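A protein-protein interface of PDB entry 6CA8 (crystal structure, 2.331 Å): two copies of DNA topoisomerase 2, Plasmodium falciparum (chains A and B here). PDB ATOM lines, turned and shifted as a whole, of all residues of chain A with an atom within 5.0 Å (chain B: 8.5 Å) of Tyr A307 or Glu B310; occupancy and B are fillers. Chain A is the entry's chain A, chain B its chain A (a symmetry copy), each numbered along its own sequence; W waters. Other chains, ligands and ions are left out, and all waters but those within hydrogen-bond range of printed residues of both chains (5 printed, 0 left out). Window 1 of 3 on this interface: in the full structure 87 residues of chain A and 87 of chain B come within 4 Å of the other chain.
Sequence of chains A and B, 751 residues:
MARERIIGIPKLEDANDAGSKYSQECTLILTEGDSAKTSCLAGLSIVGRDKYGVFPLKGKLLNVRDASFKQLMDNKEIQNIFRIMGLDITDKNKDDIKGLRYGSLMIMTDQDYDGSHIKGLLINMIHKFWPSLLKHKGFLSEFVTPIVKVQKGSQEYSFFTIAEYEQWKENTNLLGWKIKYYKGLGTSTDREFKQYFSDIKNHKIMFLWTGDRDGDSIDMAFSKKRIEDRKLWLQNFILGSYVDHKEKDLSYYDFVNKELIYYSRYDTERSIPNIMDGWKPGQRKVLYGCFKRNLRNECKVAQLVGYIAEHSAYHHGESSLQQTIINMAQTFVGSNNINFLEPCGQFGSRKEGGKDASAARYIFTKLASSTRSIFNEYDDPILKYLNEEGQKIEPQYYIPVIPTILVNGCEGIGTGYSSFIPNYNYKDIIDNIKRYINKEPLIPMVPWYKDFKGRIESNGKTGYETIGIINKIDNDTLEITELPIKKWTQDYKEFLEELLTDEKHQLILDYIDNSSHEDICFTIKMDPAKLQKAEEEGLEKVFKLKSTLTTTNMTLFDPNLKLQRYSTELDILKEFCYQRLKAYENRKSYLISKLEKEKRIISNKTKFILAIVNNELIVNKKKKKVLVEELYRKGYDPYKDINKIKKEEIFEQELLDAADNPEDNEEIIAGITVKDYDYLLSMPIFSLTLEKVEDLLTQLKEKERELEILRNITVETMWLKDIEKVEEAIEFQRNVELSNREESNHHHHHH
Of the 13 printed residues of chain A, 5 touch a printed residue of chain B.
Along chain A the printed residues that touch a printed residue of chain B span positions 293 to 310.
Of the 22 printed residues of chain B, 5 touch a printed residue of chain A.
Hydrophobic or aromatic side chains of chain B within 4 Å of the printed part of chain A: Tyr B307.
NE2 of Gln A303 is in hydrogen-bond range of OE1 of Gln B391 (3.4 Å).
OE2 of Glu B310 lies within salt-bridge range of NH1 of Arg A293 (2.7 Å).
Among the printed residues, merely in contact across the chains: Gln A303 with Glu B310, Gly A306 with Gly B306, Tyr A307 with Glu B310, Glu A310 with Gln B303 and Glu A310 with Tyr B307.
Gln A303 touches Glu B310, and with the chains exchanged Glu A310 touches Gln B303.
Gly B306 touches its own counterpart, Gly A306.
Tyr A307 touches Glu B310, and with the chains exchanged Glu A310 touches Tyr B307.
Of the 7 pairs that touch across the chains among the printed residues, 5 have their exchanged pair printed and touching as well.
Of the printed residues of chain B, Arg A293 touches Glu B310 (2.7 Å).
Of the printed residues of chain B, Gln A303 touches Glu B310 and Gln B391.
Tyr A307 touches just one residue of chain B: Glu B310.
Of the printed residues of chain B, Glu A310 touches Gln B303 and Tyr B307.
Printed residues of chain A within 4 Å of Tyr B307: Glu A310 (3.5 Å).
Glu B310 touches three residues of chain A.
Tyr B314 touches none of the printed residues of chain A.
The nearest printed residue of chain A that does not touch Gln B303 is Ala A309 (4.7 Å).
Water W1 lies within hydrogen-bond range of the side-chain amide nitrogen of Gln A303 (2.6 Å) and the side-chain amide nitrogen of Gln B653 (2.7 Å).
Water W4 bridges OE2 of Glu B310 (2.6 Å) and NH2 of Arg A293 (3.2 Å).
Water W2 lies within hydrogen-bond range of NE2 of Gln A303 (2.9 Å), OE1 of Gln B391 (3.0 Å), O of Glu B310 (3.1 Å) and N of Ala B313 (3.5 Å).
Water W3 bridges the side-chain amide nitrogen of Gln B303 (2.9 Å) and the backbone carbonyl oxygen of Glu A310 (3.1 Å).
Water W5 bridges OE1 of Glu A310 (3.1 Å) and OE1 of Glu B310 (3.1 Å).
The backbone carbonyl oxygen (O) of Glu B310 lies within hydrogen-bond range of the side-chain amide nitrogen (NE2) of Gln B391 (3.0 Å).
The backbone NH (N) of Arg A293 lies close to the side-chain hydroxyl (OH) of Tyr A307 (3.4 Å).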
ATOM      1  N   GLY A 289      -1.233  19.800 -22.824  1.00  0.00           N
ATOM      2  CA  GLY A 289      -0.752  19.341 -21.534  1.00  0.00           C
ATOM      3  C   GLY A 289      -1.435  20.073 -20.392  1.00  0.00           C
ATOM      4  O   GLY A 289      -1.808  19.459 -19.391  1.00  0.00           O
ATOM      5  N   LYS A 292      -5.038  18.758 -20.050  1.00  0.00           N
ATOM      6  CA  LYS A 292      -5.114  17.393 -19.540  1.00  0.00           C
ATOM      7  C   LYS A 292      -5.018  17.313 -18.014  1.00  0.00           C
ATOM      8  O   LYS A 292      -5.746  16.551 -17.376  1.00  0.00           O
ATOM      9  CB  LYS A 292      -4.013  16.536 -20.163  1.00  0.00           C
ATOM     10  CG  LYS A 292      -4.082  15.077 -19.751  1.00  0.00           C
ATOM     11  CD  LYS A 292      -2.940  14.266 -20.352  1.00  0.00           C
ATOM     12  CE  LYS A 292      -3.210  12.771 -20.238  1.00  0.00           C
ATOM     13  NZ  LYS A 292      -2.062  11.952 -20.703  1.00  0.00           N
ATOM     14  N   ARG A 293      -4.110  18.086 -17.431  1.00  0.00           N
ATOM     15  CA  ARG A 293      -4.001  18.140 -15.978  1.00  0.00           C
ATOM     16  C   ARG A 293      -4.936  19.178 -15.367  1.00  0.00           C
ATOM     17  O   ARG A 293      -5.036  19.285 -14.143  1.00  0.00           O
ATOM     18  CB  ARG A 293      -2.557  18.410 -15.555  1.00  0.00           C
ATOM     19  CG  ARG A 293      -2.052  19.820 -15.788  1.00  0.00           C
ATOM     20  CD  ARG A 293      -0.564  19.844 -15.501  1.00  0.00           C
ATOM     21  NE  ARG A 293      -0.310  20.189 -14.108  1.00  0.00           N
ATOM     22  CZ  ARG A 293       0.812  19.895 -13.461  1.00  0.00           C
ATOM     23  NH1 ARG A 293       1.781  19.228 -14.075  1.00  0.00           N
ATOM     24  NH2 ARG A 293       0.956  20.252 -12.191  1.00  0.00           N
ATOM     25  N   GLN A 303       8.430  22.243 -13.696  1.00  0.00           N
ATOM     26  CA  GLN A 303       7.520  21.111 -13.506  1.00  0.00           C
ATOM     27  C   GLN A 303       6.533  20.921 -14.656  1.00  0.00           C
ATOM     28  O   GLN A 303       6.271  19.787 -15.082  1.00  0.00           O
ATOM     29  CB  GLN A 303       6.774  21.265 -12.173  1.00  0.00           C
ATOM     30  CG  GLN A 303       7.686  21.530 -10.971  1.00  0.00           C
ATOM     31  CD  GLN A 303       6.915  21.812  -9.693  1.00  0.00           C
ATOM     32  OE1 GLN A 303       5.798  22.321  -9.732  1.00  0.00           O
ATOM     33  NE2 GLN A 303       7.501  21.457  -8.554  1.00  0.00           N
ATOM     34  N   LEU A 304       6.006  22.028 -15.171  1.00  0.00           N
ATOM     35  CA  LEU A 304       5.136  21.981 -16.341  1.00  0.00           C
ATOM     36  C   LEU A 304       5.892  21.416 -17.541  1.00  0.00           C
ATOM     37  O   LEU A 304       5.327  20.687 -18.355  1.00  0.00           O
ATOM     38  CB  LEU A 304       4.582  23.371 -16.666  1.00  0.00           C
ATOM     39  CG  LEU A 304       3.512  23.431 -17.761  1.00  0.00           C
ATOM     40  CD1 LEU A 304       2.397  22.424 -17.512  1.00  0.00           C
ATOM     41  CD2 LEU A 304       2.947  24.835 -17.921  1.00  0.00           C
ATOM     42  N   VAL A 305       7.173  21.759 -17.638  1.00  0.00           N
ATOM     43  CA  VAL A 305       8.033  21.282 -18.710  1.00  0.00           C
ATOM     44  C   VAL A 305       8.160  19.777 -18.638  1.00  0.00           C
ATOM     45  O   VAL A 305       7.979  19.081 -19.643  1.00  0.00           O
ATOM     46  CB  VAL A 305       9.451  21.899 -18.637  1.00  0.00           C
ATOM     47  CG1 VAL A 305      10.415  21.132 -19.538  1.00  0.00           C
ATOM     48  CG2 VAL A 305       9.426  23.373 -18.994  1.00  0.00           C
ATOM     49  N   GLY A 306       8.438  19.264 -17.442  1.00  0.00           N
ATOM     50  CA  GLY A 306       8.438  17.822 -17.279  1.00  0.00           C
ATOM     51  C   GLY A 306       7.129  17.101 -17.589  1.00  0.00           C
ATOM     52  O   GLY A 306       7.118  16.062 -18.284  1.00  0.00           O
ATOM     53  N   TYR A 307       6.012  17.687 -17.159  1.00  0.00           N
ATOM     54  CA  TYR A 307       4.700  17.119 -17.482  1.00  0.00           C
ATOM     55  C   TYR A 307       4.355  17.093 -18.972  1.00  0.00           C
ATOM     56  O   TYR A 307       3.858  16.083 -19.484  1.00  0.00           O
ATOM     57  CB  TYR A 307       3.607  17.894 -16.738  1.00  0.00           C
ATOM     58  CG  TYR A 307       2.219  17.330 -16.927  1.00  0.00           C
ATOM     59  CD1 TYR A 307       1.406  17.753 -17.975  1.00  0.00           C
ATOM     60  CD2 TYR A 307       1.717  16.375 -16.056  1.00  0.00           C
ATOM     61  CE1 TYR A 307       0.145  17.222 -18.160  1.00  0.00           C
ATOM     62  CE2 TYR A 307       0.451  15.852 -16.225  1.00  0.00           C
ATOM     63  CZ  TYR A 307      -0.331  16.276 -17.279  1.00  0.00           C
ATOM     64  OH  TYR A 307      -1.598  15.761 -17.439  1.00  0.00           O
ATOM     65  N   ILE A 308       4.615  18.200 -19.661  1.00  0.00           N
ATOM     66  CA  ILE A 308       4.404  18.271 -21.105  1.00  0.00           C
ATOM     67  C   ILE A 308       5.316  17.307 -21.852  1.00  0.00           C
ATOM     68  O   ILE A 308       4.887  16.652 -22.799  1.00  0.00           O
ATOM     69  CB  ILE A 308       4.596  19.698 -21.659  1.00  0.00           C
ATOM     70  CG1 ILE A 308       3.541  20.642 -21.080  1.00  0.00           C
ATOM     71  CG2 ILE A 308       4.455  19.710 -23.168  1.00  0.00           C
ATOM     72  CD1 ILE A 308       4.003  22.071 -20.964  1.00  0.00           C
ATOM     73  N   ALA A 309       6.576  17.231 -21.443  1.00  0.00           N
ATOM     74  CA  ALA A 309       7.492  16.308 -22.096  1.00  0.00           C
ATOM     75  C   ALA A 309       6.977  14.873 -21.978  1.00  0.00           C
ATOM     76  O   ALA A 309       7.021  14.115 -22.951  1.00  0.00           O
ATOM     77  CB  ALA A 309       8.890  16.429 -21.508  1.00  0.00           C
ATOM     78  N   GLU A 310       6.484  14.490 -20.802  1.00  0.00           N
ATOM     79  CA  GLU A 310       5.846  13.172 -20.701  1.00  0.00           C
ATOM     80  C   GLU A 310       4.541  12.961 -21.491  1.00  0.00           C
ATOM     81  O   GLU A 310       4.370  11.925 -22.131  1.00  0.00           O
ATOM     82  CB  GLU A 310       5.573  12.808 -19.242  1.00  0.00           C
ATOM     83  CG  GLU A 310       5.367  11.305 -19.075  1.00  0.00           C
ATOM     84  CD  GLU A 310       5.017  10.890 -17.669  1.00  0.00           C
ATOM     85  OE1 GLU A 310       5.054  11.748 -16.767  1.00  0.00           O
ATOM     86  OE2 GLU A 310       4.712   9.697 -17.465  1.00  0.00           O
ATOM     87  N   HIS A 311       3.626  13.927 -21.452  1.00  0.00           N
ATOM     88  CA  HIS A 311       2.260  13.708 -21.950  1.00  0.00           C
ATOM     89  C   HIS A 311       1.942  14.198 -23.367  1.00  0.00           C
ATOM     90  O   HIS A 311       0.930  13.803 -23.948  1.00  0.00           O
ATOM     91  CB  HIS A 311       1.269  14.336 -20.969  1.00  0.00           C
ATOM     92  CG  HIS A 311       1.258  13.672 -19.628  1.00  0.00           C
ATOM     93  ND1 HIS A 311       0.507  12.548 -19.356  1.00  0.00           N
ATOM     94  CD2 HIS A 311       1.933  13.958 -18.491  1.00  0.00           C
ATOM     95  CE1 HIS A 311       0.706  12.182 -18.102  1.00  0.00           C
ATOM     96  NE2 HIS A 311       1.568  13.021 -17.555  1.00  0.00           N
ATOM     97  N   SER A 312       2.794  15.052 -23.919  1.00  0.00           N
ATOM     98  CA  SER A 312       2.536  15.654 -25.223  1.00  0.00           C
ATOM     99  C   SER A 312       3.540  15.217 -26.290  1.00  0.00           C
ATOM    100  O   SER A 312       3.450  15.645 -27.444  1.00  0.00           O
ATOM    101  CB  SER A 312       2.532  17.178 -25.108  1.00  0.00           C
ATOM    102  OG  SER A 312       1.588  17.622 -24.149  1.00  0.00           O
ATOM    103  N   TYR B 288      13.046   7.499  -6.196  1.00  0.00           N
ATOM    104  CA  TYR B 288      11.855   8.024  -5.539  1.00  0.00           C
ATOM    105  C   TYR B 288      10.734   8.269  -6.546  1.00  0.00           C
ATOM    106  O   TYR B 288       9.572   7.926  -6.292  1.00  0.00           O
ATOM    107  CB  TYR B 288      12.184   9.313  -4.784  1.00  0.00           C
ATOM    108  CG  TYR B 288      10.967  10.070  -4.308  1.00  0.00           C
ATOM    109  CD1 TYR B 288      10.212   9.606  -3.237  1.00  0.00           C
ATOM    110  CD2 TYR B 288      10.565  11.245  -4.932  1.00  0.00           C
ATOM    111  CE1 TYR B 288       9.092  10.291  -2.800  1.00  0.00           C
ATOM    112  CE2 TYR B 288       9.447  11.937  -4.499  1.00  0.00           C
ATOM    113  CZ  TYR B 288       8.716  11.458  -3.434  1.00  0.00           C
ATOM    114  OH  TYR B 288       7.606  12.146  -2.996  1.00  0.00           O
ATOM    115  N   GLY B 289      11.092   8.848  -7.692  1.00  0.00           N
ATOM    116  CA  GLY B 289      10.114   9.085  -8.737  1.00  0.00           C
ATOM    117  C   GLY B 289       9.522   7.785  -9.252  1.00  0.00           C
ATOM    118  O   GLY B 289       8.314   7.694  -9.475  1.00  0.00           O
ATOM    119  N   LYS B 292       7.077   6.402  -6.620  1.00  0.00           N
ATOM    120  CA  LYS B 292       5.853   7.188  -6.491  1.00  0.00           C
ATOM    121  C   LYS B 292       4.799   6.841  -7.546  1.00  0.00           C
ATOM    122  O   LYS B 292       3.609   6.748  -7.241  1.00  0.00           O
ATOM    123  CB  LYS B 292       6.175   8.679  -6.568  1.00  0.00           C
ATOM    124  CG  LYS B 292       4.964   9.568  -6.351  1.00  0.00           C
ATOM    125  CD  LYS B 292       5.316  11.044  -6.484  1.00  0.00           C
ATOM    126  CE  LYS B 292       4.207  11.925  -5.920  1.00  0.00           C
ATOM    127  NZ  LYS B 292       4.464  13.371  -6.145  1.00  0.00           N
ATOM    128  N   ALA B 302      12.754   9.285 -21.720  1.00  0.00           N
ATOM    129  CA  ALA B 302      12.417  10.709 -21.821  1.00  0.00           C
ATOM    130  C   ALA B 302      11.148  11.132 -21.061  1.00  0.00           C
ATOM    131  O   ALA B 302      11.130  12.172 -20.373  1.00  0.00           O
ATOM    132  CB  ALA B 302      12.286  11.097 -23.292  1.00  0.00           C
ATOM    133  N   GLN B 303      10.126  10.283 -21.095  1.00  0.00           N
ATOM    134  CA  GLN B 303       8.942  10.482 -20.256  1.00  0.00           C
ATOM    135  C   GLN B 303       9.226  10.358 -18.760  1.00  0.00           C
ATOM    136  O   GLN B 303       8.713  11.147 -17.953  1.00  0.00           O
ATOM    137  CB  GLN B 303       7.837   9.503 -20.679  1.00  0.00           C
ATOM    138  CG  GLN B 303       7.535   9.510 -22.181  1.00  0.00           C
ATOM    139  CD  GLN B 303       6.538   8.439 -22.589  1.00  0.00           C
ATOM    140  OE1 GLN B 303       6.446   7.391 -21.956  1.00  0.00           O
ATOM    141  NE2 GLN B 303       5.769   8.712 -23.638  1.00  0.00           N
ATOM    142  N   LEU B 304      10.058   9.388 -18.395  1.00  0.00           N
ATOM    143  CA  LEU B 304      10.490   9.239 -17.010  1.00  0.00           C
ATOM    144  C   LEU B 304      11.252  10.481 -16.556  1.00  0.00           C
ATOM    145  O   LEU B 304      11.137  10.906 -15.408  1.00  0.00           O
ATOM    146  CB  LEU B 304      11.357   7.989 -16.838  1.00  0.00           C
ATOM    147  CG  LEU B 304      11.726   7.615 -15.399  1.00  0.00           C
ATOM    148  CD1 LEU B 304      10.500   7.579 -14.497  1.00  0.00           C
ATOM    149  CD2 LEU B 304      12.486   6.299 -15.334  1.00  0.00           C
ATOM    150  N   VAL B 305      12.029  11.056 -17.471  1.00  0.00           N
ATOM    151  CA  VAL B 305      12.799  12.260 -17.200  1.00  0.00           C
ATOM    152  C   VAL B 305      11.867  13.405 -16.877  1.00  0.00           C
ATOM    153  O   VAL B 305      12.052  14.104 -15.874  1.00  0.00           O
ATOM    154  CB  VAL B 305      13.682  12.669 -18.405  1.00  0.00           C
ATOM    155  CG1 VAL B 305      14.196  14.095 -18.231  1.00  0.00           C
ATOM    156  CG2 VAL B 305      14.828  11.694 -18.599  1.00  0.00           C
ATOM    157  N   GLY B 306      10.841  13.584 -17.705  1.00  0.00           N
ATOM    158  CA  GLY B 306       9.837  14.579 -17.375  1.00  0.00           C
ATOM    159  C   GLY B 306       9.094  14.385 -16.055  1.00  0.00           C
ATOM    160  O   GLY B 306       8.921  15.342 -15.270  1.00  0.00           O
ATOM    161  N   TYR B 307       8.730  13.139 -15.757  1.00  0.00           N
ATOM    162  CA  TYR B 307       8.090  12.836 -14.474  1.00  0.00           C
ATOM    163  C   TYR B 307       8.957  13.095 -13.240  1.00  0.00           C
ATOM    164  O   TYR B 307       8.487  13.674 -12.254  1.00  0.00           O
ATOM    165  CB  TYR B 307       7.637  11.371 -14.458  1.00  0.00           C
ATOM    166  CG  TYR B 307       6.877  10.978 -13.213  1.00  0.00           C
ATOM    167  CD1 TYR B 307       7.540  10.488 -12.091  1.00  0.00           C
ATOM    168  CD2 TYR B 307       5.497  11.093 -13.159  1.00  0.00           C
ATOM    169  CE1 TYR B 307       6.848  10.148 -10.946  1.00  0.00           C
ATOM    170  CE2 TYR B 307       4.797  10.740 -12.023  1.00  0.00           C
ATOM    171  CZ  TYR B 307       5.475  10.269 -10.918  1.00  0.00           C
ATOM    172  OH  TYR B 307       4.774   9.906  -9.790  1.00  0.00           O
ATOM    173  N   ILE B 308      10.213  12.664 -13.297  1.00  0.00           N
ATOM    174  CA  ILE B 308      11.161  12.921 -12.216  1.00  0.00           C
ATOM    175  C   ILE B 308      11.428  14.411 -12.048  1.00  0.00           C
ATOM    176  O   ILE B 308      11.502  14.908 -10.927  1.00  0.00           O
ATOM    177  CB  ILE B 308      12.497  12.176 -12.413  1.00  0.00           C
ATOM    178  CG1 ILE B 308      12.277  10.663 -12.365  1.00  0.00           C
ATOM    179  CG2 ILE B 308      13.479  12.540 -11.318  1.00  0.00           C
ATOM    180  CD1 ILE B 308      13.261   9.880 -13.192  1.00  0.00           C
ATOM    181  N   ALA B 309      11.591  15.122 -13.157  1.00  0.00           N
ATOM    182  CA  ALA B 309      11.820  16.556 -13.067  1.00  0.00           C
ATOM    183  C   ALA B 309      10.652  17.240 -12.357  1.00  0.00           C
ATOM    184  O   ALA B 309      10.863  18.112 -11.510  1.00  0.00           O
ATOM    185  CB  ALA B 309      12.037  17.155 -14.449  1.00  0.00           C
ATOM    186  N   GLU B 310       9.421  16.854 -12.685  1.00  0.00           N
ATOM    187  CA  GLU B 310       8.288  17.383 -11.916  1.00  0.00           C
ATOM    188  C   GLU B 310       8.189  16.968 -10.436  1.00  0.00           C
ATOM    189  O   GLU B 310       7.919  17.807  -9.578  1.00  0.00           O
ATOM    190  CB  GLU B 310       6.960  17.033 -12.588  1.00  0.00           C
ATOM    191  CG  GLU B 310       5.837  17.942 -12.101  1.00  0.00           C
ATOM    192  CD  GLU B 310       4.484  17.598 -12.670  1.00  0.00           C
ATOM    193  OE1 GLU B 310       4.413  16.726 -13.555  1.00  0.00           O
ATOM    194  OE2 GLU B 310       3.487  18.211 -12.234  1.00  0.00           O
ATOM    195  N   HIS B 311       8.406  15.690 -10.131  1.00  0.00           N
ATOM    196  CA  HIS B 311       8.080  15.155  -8.802  1.00  0.00           C
ATOM    197  C   HIS B 311       9.227  15.034  -7.792  1.00  0.00           C
ATOM    198  O   HIS B 311       8.987  14.871  -6.595  1.00  0.00           O
ATOM    199  CB  HIS B 311       7.414  13.788  -8.968  1.00  0.00           C
ATOM    200  CG  HIS B 311       6.083  13.853  -9.649  1.00  0.00           C
ATOM    201  ND1 HIS B 311       4.910  14.119  -8.975  1.00  0.00           N
ATOM    202  CD2 HIS B 311       5.746  13.719 -10.953  1.00  0.00           C
ATOM    203  CE1 HIS B 311       3.905  14.126  -9.833  1.00  0.00           C
ATOM    204  NE2 HIS B 311       4.385  13.885 -11.040  1.00  0.00           N
ATOM    205  N   SER B 312      10.463  15.111  -8.267  1.00  0.00           N
ATOM    206  CA  SER B 312      11.626  14.913  -7.407  1.00  0.00           C
ATOM    207  C   SER B 312      12.474  16.176  -7.252  1.00  0.00           C
ATOM    208  O   SER B 312      13.491  16.162  -6.554  1.00  0.00           O
ATOM    209  CB  SER B 312      12.489  13.772  -7.945  1.00  0.00           C
ATOM    210  OG  SER B 312      11.744  12.575  -8.073  1.00  0.00           O
ATOM    211  N   ALA B 313      12.049  17.259  -7.899  1.00  0.00           N
ATOM    212  CA  ALA B 313      12.786  18.525  -7.896  1.00  0.00           C
ATOM    213  C   ALA B 313      14.241  18.390  -8.336  1.00  0.00           C
ATOM    214  O   ALA B 313      15.159  18.807  -7.626  1.00  0.00           O
ATOM    215  CB  ALA B 313      12.721  19.167  -6.511  1.00  0.00           C
ATOM    216  N   TYR B 314      14.450  17.793  -9.503  1.00  0.00           N
ATOM    217  CA  TYR B 314      15.789  17.671 -10.051  1.00  0.00           C
ATOM    218  C   TYR B 314      16.094  18.935 -10.856  1.00  0.00           C
ATOM    219  O   TYR B 314      15.354  19.273 -11.780  1.00  0.00           O
ATOM    220  CB  TYR B 314      15.876  16.426 -10.935  1.00  0.00           C
ATOM    221  CG  TYR B 314      17.253  16.118 -11.457  1.00  0.00           C
ATOM    222  CD1 TYR B 314      18.142  15.369 -10.704  1.00  0.00           C
ATOM    223  CD2 TYR B 314      17.672  16.586 -12.693  1.00  0.00           C
ATOM    224  CE1 TYR B 314      19.408  15.083 -11.170  1.00  0.00           C
ATOM    225  CE2 TYR B 314      18.936  16.307 -13.169  1.00  0.00           C
ATOM    226  CZ  TYR B 314      19.802  15.556 -12.402  1.00  0.00           C
ATOM    227  OH  TYR B 314      21.062  15.269 -12.866  1.00  0.00           O
ATOM    228  N   HIS B 315      17.174  19.634 -10.510  1.00  0.00           N
ATOM    229  CA  HIS B 315      17.477  20.925 -11.143  1.00  0.00           C
ATOM    230  C   HIS B 315      18.705  21.008 -12.052  1.00  0.00           C
ATOM    231  O   HIS B 315      19.079  22.102 -12.470  1.00  0.00           O
ATOM    232  CB  HIS B 315      17.616  22.014 -10.077  1.00  0.00           C
ATOM    233  CG  HIS B 315      16.562  21.970  -9.017  1.00  0.00           C
ATOM    234  ND1 HIS B 315      15.237  22.245  -9.279  1.00  0.00           N
ATOM    235  CD2 HIS B 315      16.641  21.721  -7.689  1.00  0.00           C
ATOM    236  CE1 HIS B 315      14.541  22.147  -8.161  1.00  0.00           C
ATOM    237  NE2 HIS B 315      15.368  21.832  -7.180  1.00  0.00           N
ATOM    238  N   LEU B 321      19.934  14.147 -16.041  1.00  0.00           N
ATOM    239  CA  LEU B 321      18.873  13.248 -15.589  1.00  0.00           C
ATOM    240  C   LEU B 321      18.716  11.969 -16.431  1.00  0.00           C
ATOM    241  O   LEU B 321      18.599  10.852 -15.892  1.00  0.00           O
ATOM    242  CB  LEU B 321      17.546  14.016 -15.562  1.00  0.00           C
ATOM    243  CG  LEU B 321      16.362  13.387 -14.840  1.00  0.00           C
ATOM    244  CD1 LEU B 321      16.814  12.821 -13.501  1.00  0.00           C
ATOM    245  CD2 LEU B 321      15.272  14.430 -14.652  1.00  0.00           C
ATOM    246  N   GLN B 391       6.843  21.112  -1.441  1.00  0.00           N
ATOM    247  CA  GLN B 391       6.675  19.840  -2.136  1.00  0.00           C
ATOM    248  C   GLN B 391       7.410  18.707  -1.423  1.00  0.00           C
ATOM    249  O   GLN B 391       8.562  18.859  -1.017  1.00  0.00           O
ATOM    250  CB  GLN B 391       7.149  19.952  -3.584  1.00  0.00           C
ATOM    251  CG  GLN B 391       7.004  18.669  -4.390  1.00  0.00           C
ATOM    252  CD  GLN B 391       7.608  18.783  -5.778  1.00  0.00           C
ATOM    253  OE1 GLN B 391       8.588  19.501  -5.986  1.00  0.00           O
ATOM    254  NE2 GLN B 391       7.021  18.077  -6.738  1.00  0.00           N
ATOM    255  N   LYS B 392       6.736  17.571  -1.277  1.00  0.00           N
ATOM    256  CA  LYS B 392       7.363  16.392  -0.699  1.00  0.00           C
ATOM    257  C   LYS B 392       8.191  15.679  -1.758  1.00  0.00           C
ATOM    258  O   LYS B 392       7.650  15.138  -2.721  1.00  0.00           O
ATOM    259  CB  LYS B 392       6.292  15.448  -0.146  1.00  0.00           C
ATOM    260  CG  LYS B 392       6.803  14.138   0.437  1.00  0.00           C
ATOM    261  CD  LYS B 392       5.632  13.186   0.676  1.00  0.00           C
ATOM    262  CE  LYS B 392       5.882  12.240   1.836  1.00  0.00           C
ATOM    263  NZ  LYS B 392       6.355  10.908   1.361  1.00  0.00           N
ATOM    264  N   ILE B 393       9.505  15.666  -1.563  1.00  0.00           N
ATOM    265  CA  ILE B 393      10.426  15.043  -2.511  1.00  0.00           C
ATOM    266  C   ILE B 393      11.106  13.806  -1.925  1.00  0.00           C
ATOM    267  O   ILE B 393      10.593  13.194  -0.987  1.00  0.00           O
ATOM    268  CB  ILE B 393      11.479  16.055  -3.020  1.00  0.00           C
ATOM    269  CG1 ILE B 393      12.078  16.854  -1.862  1.00  0.00           C
ATOM    270  CG2 ILE B 393      10.851  17.010  -4.016  1.00  0.00           C
ATOM    271  CD1 ILE B 393      13.285  17.684  -2.254  1.00  0.00           C
ATOM    272  N   GLN B 653       1.900  21.047  -0.356  1.00  0.00           N
ATOM    273  CA  GLN B 653       1.295  20.838  -1.669  1.00  0.00           C
ATOM    274  C   GLN B 653       0.394  19.608  -1.699  1.00  0.00           C
ATOM    275  O   GLN B 653      -0.124  19.225  -2.747  1.00  0.00           O
ATOM    276  CB  GLN B 653       2.378  20.747  -2.744  1.00  0.00           C
ATOM    277  CG  GLN B 653       3.196  22.026  -2.854  1.00  0.00           C
ATOM    278  CD  GLN B 653       3.985  22.119  -4.139  1.00  0.00           C
ATOM    279  OE1 GLN B 653       3.653  21.479  -5.135  1.00  0.00           O
ATOM    280  NE2 GLN B 653       5.036  22.927  -4.126  1.00  0.00           N
HETATM  281  O   HOH W   1       6.014  21.932  -6.455  1.00  0.00           O
HETATM  282  O   HOH W   2       9.939  19.961  -8.584  1.00  0.00           O
HETATM  283  O   HOH W   3       5.809  11.314 -24.827  1.00  0.00           O
HETATM  284  O   HOH W   4       3.408  19.788 -10.144  1.00  0.00           O
HETATM  285  O   HOH W   5       5.286  14.483 -15.433  1.00  0.00           O
